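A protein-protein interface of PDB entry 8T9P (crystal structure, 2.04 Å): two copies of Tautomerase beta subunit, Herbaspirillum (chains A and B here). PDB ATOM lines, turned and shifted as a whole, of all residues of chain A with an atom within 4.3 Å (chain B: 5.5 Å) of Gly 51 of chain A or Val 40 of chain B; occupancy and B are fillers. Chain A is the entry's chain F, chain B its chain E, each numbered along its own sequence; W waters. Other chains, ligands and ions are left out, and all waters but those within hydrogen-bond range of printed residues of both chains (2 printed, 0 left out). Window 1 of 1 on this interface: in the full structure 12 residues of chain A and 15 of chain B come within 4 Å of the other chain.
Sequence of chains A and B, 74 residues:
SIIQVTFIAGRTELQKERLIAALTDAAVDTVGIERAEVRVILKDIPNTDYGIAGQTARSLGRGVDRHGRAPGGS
N of Leu 42 of chain B is in hydrogen-bond range of O of Asp 49 of chain A (3.1 Å). The backbone NH (N) of Gly 51 of chain A is in hydrogen-bond range of the backbone carbonyl oxygen (O) of Val 40 of chain B, 2.8 Å away. O of Val 38 of chain B lies within hydrogen-bond range of N of Ala 53 of chain A, at 3.2 Å.
The backbone carbonyl oxygen (O) of Arg 39 of chain B lies within hydrogen-bond range of the backbone NH (N) of Ile 3 of chain B, at 2.8 Å. The backbone NH (N) of Ile 41 of chain B is in hydrogen-bond range of the backbone carbonyl oxygen (O) of Ile 3 of chain B (2.7 Å). N of Val 5 of chain B lies within hydrogen-bond range of O of Ile 41 of chain B, 2.7 Å away. OG1 of Thr 24 of chain B is in hydrogen-bond range of O of Ile 20 of chain B.
Asp 49 of chain A touches Val 40 of chain B (O to O, 3.8 Å). OH of Tyr 50 of chain A touches CD of Arg 39 of chain B, at 3.1 Å. O of Val 40 of chain B touches CD1 of Tyr 50 of chain A (3.1 Å). CD1 of Tyr 50 of chain A touches CD1 of Ile 41 of chain B, 3.2 Å away. CA of Gly 51 of chain A touches CG2 of Ile 20 of chain B, at 3.6 Å. Gly 51 of chain A touches Val 38 of chain B. Gly 51 of chain A touches Arg 39 of chain B. O of Val 38 of chain B touches CA of Ile 52 of chain A (3.9 Å). Ile 20 of chain B touches Gln 55 of chain A.
Gly 51 of chain A touches just these residues of chain B: Ile 20, Val 38, Arg 39 and Val 40. Val 40 of chain B touches just these residues of chain A: Asp 49 (3.8 Å), Tyr 50 (3.1 Å) and Gly 51 (2.8 Å). Of the printed residues of chain B, Asp 49 of chain A touches Val 40 and Leu 42. Of the printed residues of chain A, Ile 20 of chain B touches Gly 51 and Gln 55. Leu 23 of chain B touches none of the printed residues of chain A. Ile 3 of chain B touches none of the printed residues of chain A. The nearest printed residue of chain A that does not touch Ile 41 of chain B is Asp 49 of chain A (4.04 Å).
Hydrophobic or aromatic side chains of chain B that line the printed part of chain A: Ile 20, Ile 41 and Leu 42. Among the printed residues, no Asp or Glu carboxylate lies within 4 Å of a Lys or Arg side-chain nitrogen of the other chain.
No position is printed for both chains.
Water W1 bridges O of Leu 42 of chain B (2.6 Å) and OD2 of Asp 49 of chain A (2.8 Å). Water W2 lies within hydrogen-bond range of O of Val 38 of chain B, OG1 of Thr 24 of chain B and N of Ala 53 of chain A.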
ATOM      1  N   ASP A  49       0.180  -3.908  14.557  1.00  0.00           N
ATOM      2  CA  ASP A  49       1.577  -3.867  14.972  1.00  0.00           C
ATOM      3  C   ASP A  49       1.935  -4.944  15.980  1.00  0.00           C
ATOM      4  O   ASP A  49       3.032  -4.890  16.558  1.00  0.00           O
ATOM      5  CB  ASP A  49       1.962  -2.507  15.572  1.00  0.00           C
ATOM      6  CG  ASP A  49       1.667  -1.361  14.629  1.00  0.00           C
ATOM      7  OD1 ASP A  49       1.522  -1.617  13.404  1.00  0.00           O
ATOM      8  OD2 ASP A  49       1.701  -0.203  15.048  1.00  0.00           O
ATOM      9  N   TYR A  50       1.062  -5.919  16.227  1.00  0.00           N
ATOM     10  CA  TYR A  50       1.412  -6.938  17.210  1.00  0.00           C
ATOM     11  C   TYR A  50       1.235  -8.352  16.703  1.00  0.00           C
ATOM     12  O   TYR A  50       0.174  -8.731  16.197  1.00  0.00           O
ATOM     13  CB  TYR A  50       0.730  -6.641  18.552  1.00  0.00           C
ATOM     14  CG  TYR A  50       0.810  -7.644  19.677  1.00  0.00           C
ATOM     15  CD1 TYR A  50       1.915  -8.446  19.876  1.00  0.00           C
ATOM     16  CD2 TYR A  50       0.122  -7.324  20.829  1.00  0.00           C
ATOM     17  CE1 TYR A  50       2.029  -9.260  21.023  1.00  0.00           C
ATOM     18  CE2 TYR A  50       0.261  -8.041  22.005  1.00  0.00           C
ATOM     19  CZ  TYR A  50       1.218  -9.001  22.105  1.00  0.00           C
ATOM     20  OH  TYR A  50       1.335  -9.696  23.285  1.00  0.00           O
ATOM     21  N   GLY A  51       2.341  -9.086  16.783  1.00  0.00           N
ATOM     22  CA  GLY A  51       2.458 -10.406  16.214  1.00  0.00           C
ATOM     23  C   GLY A  51       2.287 -11.472  17.288  1.00  0.00           C
ATOM     24  O   GLY A  51       2.801 -11.343  18.401  1.00  0.00           O
ATOM     25  N   ILE A  52       1.542 -12.504  16.924  1.00  0.00           N
ATOM     26  CA  ILE A  52       1.324 -13.684  17.746  1.00  0.00           C
ATOM     27  C   ILE A  52       1.564 -14.878  16.837  1.00  0.00           C
ATOM     28  O   ILE A  52       0.876 -15.029  15.820  1.00  0.00           O
ATOM     29  CB  ILE A  52      -0.098 -13.718  18.330  1.00  0.00           C
ATOM     30  CG1 ILE A  52      -0.300 -12.540  19.290  1.00  0.00           C
ATOM     31  CG2 ILE A  52      -0.375 -15.054  19.010  1.00  0.00           C
ATOM     32  CD1 ILE A  52      -1.679 -11.941  19.223  1.00  0.00           C
ATOM     33  N   ALA A  53       2.573 -15.683  17.167  1.00  0.00           N
ATOM     34  CA  ALA A  53       2.898 -16.889  16.415  1.00  0.00           C
ATOM     35  C   ALA A  53       3.231 -16.583  14.955  1.00  0.00           C
ATOM     36  O   ALA A  53       3.034 -17.424  14.079  1.00  0.00           O
ATOM     37  CB  ALA A  53       1.765 -17.920  16.503  1.00  0.00           C
ATOM     38  N   GLN A  55       1.820 -14.073  13.177  1.00  0.00           N
ATOM     39  CA  GLN A  55       0.691 -13.420  12.531  1.00  0.00           C
ATOM     40  C   GLN A  55       0.323 -12.157  13.290  1.00  0.00           C
ATOM     41  O   GLN A  55       0.505 -12.073  14.505  1.00  0.00           O
ATOM     42  CB  GLN A  55      -0.544 -14.331  12.496  1.00  0.00           C
ATOM     43  CG  GLN A  55      -0.433 -15.526  11.579  1.00  0.00           C
ATOM     44  CD  GLN A  55      -1.740 -16.279  11.510  1.00  0.00           C
ATOM     45  OE1 GLN A  55      -1.913 -17.304  12.171  1.00  0.00           O
ATOM     46  NE2 GLN A  55      -2.678 -15.765  10.723  1.00  0.00           N
ATOM     47  N   ILE B   3       9.638 -10.109  21.472  1.00  0.00           N
ATOM     48  CA  ILE B   3      10.517  -9.345  20.591  1.00  0.00           C
ATOM     49  C   ILE B   3       9.925  -7.947  20.454  1.00  0.00           C
ATOM     50  O   ILE B   3       8.794  -7.796  19.982  1.00  0.00           O
ATOM     51  CB  ILE B   3      10.671 -10.028  19.221  1.00  0.00           C
ATOM     52  CG1 ILE B   3      11.194 -11.458  19.391  1.00  0.00           C
ATOM     53  CG2 ILE B   3      11.680  -9.277  18.393  1.00  0.00           C
ATOM     54  CD1 ILE B   3      11.111 -12.282  18.090  1.00  0.00           C
ATOM     55  N   VAL B   5      10.360  -4.194  18.812  1.00  0.00           N
ATOM     56  CA  VAL B   5      11.020  -3.497  17.718  1.00  0.00           C
ATOM     57  C   VAL B   5      10.650  -2.036  17.810  1.00  0.00           C
ATOM     58  O   VAL B   5       9.466  -1.696  17.881  1.00  0.00           O
ATOM     59  CB  VAL B   5      10.628  -4.057  16.334  1.00  0.00           C
ATOM     60  CG1 VAL B   5      11.078  -3.105  15.242  1.00  0.00           C
ATOM     61  CG2 VAL B   5      11.225  -5.431  16.115  1.00  0.00           C
ATOM     62  N   LEU B  19       7.798  -8.332   8.634  1.00  0.00           N
ATOM     63  CA  LEU B  19       8.734  -8.266   9.753  1.00  0.00           C
ATOM     64  C   LEU B  19       8.321  -9.218  10.866  1.00  0.00           C
ATOM     65  O   LEU B  19       9.142  -9.981  11.380  1.00  0.00           O
ATOM     66  CB  LEU B  19       8.776  -6.842  10.286  1.00  0.00           C
ATOM     67  CG  LEU B  19       9.894  -6.450  11.250  1.00  0.00           C
ATOM     68  CD1 LEU B  19      11.258  -6.753  10.649  1.00  0.00           C
ATOM     69  CD2 LEU B  19       9.772  -4.981  11.653  1.00  0.00           C
ATOM     70  N   ILE B  20       7.049  -9.166  11.271  1.00  0.00           N
ATOM     71  CA  ILE B  20       6.544 -10.051  12.320  1.00  0.00           C
ATOM     72  C   ILE B  20       6.843 -11.495  11.958  1.00  0.00           C
ATOM     73  O   ILE B  20       7.351 -12.266  12.780  1.00  0.00           O
ATOM     74  CB  ILE B  20       5.033  -9.818  12.516  1.00  0.00           C
ATOM     75  CG1 ILE B  20       4.802  -8.522  13.293  1.00  0.00           C
ATOM     76  CG2 ILE B  20       4.399 -11.024  13.206  1.00  0.00           C
ATOM     77  CD1 ILE B  20       3.425  -7.912  13.067  1.00  0.00           C
ATOM     78  N   LEU B  23      10.884 -12.173  11.856  1.00  0.00           N
ATOM     79  CA  LEU B  23      11.489 -12.244  13.185  1.00  0.00           C
ATOM     80  C   LEU B  23      11.046 -13.496  13.926  1.00  0.00           C
ATOM     81  O   LEU B  23      11.841 -14.118  14.643  1.00  0.00           O
ATOM     82  CB  LEU B  23      11.145 -10.995  14.003  1.00  0.00           C
ATOM     83  CG  LEU B  23      11.719  -9.665  13.512  1.00  0.00           C
ATOM     84  CD1 LEU B  23      10.921  -8.482  14.075  1.00  0.00           C
ATOM     85  CD2 LEU B  23      13.204  -9.580  13.861  1.00  0.00           C
ATOM     86  N   THR B  24       9.780 -13.880  13.768  1.00  0.00           N
ATOM     87  CA  THR B  24       9.306 -15.093  14.427  1.00  0.00           C
ATOM     88  C   THR B  24       9.993 -16.328  13.863  1.00  0.00           C
ATOM     89  O   THR B  24      10.424 -17.205  14.625  1.00  0.00           O
ATOM     90  CB  THR B  24       7.789 -15.210  14.297  1.00  0.00           C
ATOM     91  OG1 THR B  24       7.173 -14.006  14.769  1.00  0.00           O
ATOM     92  CG2 THR B  24       7.269 -16.405  15.099  1.00  0.00           C
ATOM     93  N   VAL B  38       5.911 -16.964  20.566  1.00  0.00           N
ATOM     94  CA  VAL B  38       6.700 -15.795  20.188  1.00  0.00           C
ATOM     95  C   VAL B  38       5.770 -14.604  20.018  1.00  0.00           C
ATOM     96  O   VAL B  38       4.842 -14.636  19.205  1.00  0.00           O
ATOM     97  CB  VAL B  38       7.493 -16.046  18.898  1.00  0.00           C
ATOM     98  CG1 VAL B  38       8.186 -14.756  18.464  1.00  0.00           C
ATOM     99  CG2 VAL B  38       8.510 -17.145  19.108  1.00  0.00           C
ATOM    100  N   ARG B  39       6.025 -13.541  20.770  1.00  0.00           N
ATOM    101  CA  ARG B  39       5.292 -12.294  20.630  1.00  0.00           C
ATOM    102  C   ARG B  39       6.195 -11.256  19.978  1.00  0.00           C
ATOM    103  O   ARG B  39       7.385 -11.174  20.293  1.00  0.00           O
ATOM    104  CB  ARG B  39       4.802 -11.795  21.991  1.00  0.00           C
ATOM    105  CG  ARG B  39       3.467 -12.371  22.397  1.00  0.00           C
ATOM    106  CD  ARG B  39       3.156 -12.104  23.861  1.00  0.00           C
ATOM    107  NE  ARG B  39       2.170 -13.054  24.361  1.00  0.00           N
ATOM    108  CZ  ARG B  39       1.456 -12.887  25.467  1.00  0.00           C
ATOM    109  NH1 ARG B  39       1.618 -11.801  26.213  1.00  0.00           N
ATOM    110  NH2 ARG B  39       0.593 -13.824  25.832  1.00  0.00           N
ATOM    111  N   VAL B  40       5.640 -10.477  19.059  1.00  0.00           N
ATOM    112  CA  VAL B  40       6.394  -9.422  18.392  1.00  0.00           C
ATOM    113  C   VAL B  40       5.642  -8.118  18.600  1.00  0.00           C
ATOM    114  O   VAL B  40       4.472  -8.000  18.220  1.00  0.00           O
ATOM    115  CB  VAL B  40       6.616  -9.720  16.897  1.00  0.00           C
ATOM    116  CG1 VAL B  40       7.160  -8.489  16.180  1.00  0.00           C
ATOM    117  CG2 VAL B  40       7.588 -10.874  16.732  1.00  0.00           C
ATOM    118  N   ILE B  41       6.304  -7.157  19.236  1.00  0.00           N
ATOM    119  CA  ILE B  41       5.758  -5.840  19.531  1.00  0.00           C
ATOM    120  C   ILE B  41       6.493  -4.851  18.643  1.00  0.00           C
ATOM    121  O   ILE B  41       7.709  -4.677  18.783  1.00  0.00           O
ATOM    122  CB  ILE B  41       5.974  -5.458  21.009  1.00  0.00           C
ATOM    123  CG1 ILE B  41       5.351  -6.469  21.960  1.00  0.00           C
ATOM    124  CG2 ILE B  41       5.436  -4.078  21.271  1.00  0.00           C
ATOM    125  CD1 ILE B  41       3.995  -6.771  21.640  1.00  0.00           C
ATOM    126  N   LEU B  42       5.767  -4.192  17.757  1.00  0.00           N
ATOM    127  CA  LEU B  42       6.338  -3.176  16.889  1.00  0.00           C
ATOM    128  C   LEU B  42       5.945  -1.816  17.442  1.00  0.00           C
ATOM    129  O   LEU B  42       4.762  -1.550  17.669  1.00  0.00           O
ATOM    130  CB  LEU B  42       5.851  -3.351  15.446  1.00  0.00           C
ATOM    131  CG  LEU B  42       6.053  -4.730  14.798  1.00  0.00           C
ATOM    132  CD1 LEU B  42       5.566  -4.713  13.336  1.00  0.00           C
ATOM    133  CD2 LEU B  42       7.508  -5.136  14.870  1.00  0.00           C
HETATM  134  O   HOH W   1       3.463   0.598  17.122  1.00  0.00           O
HETATM  135  O   HOH W   2       4.956 -13.617  16.549  1.00  0.00           O
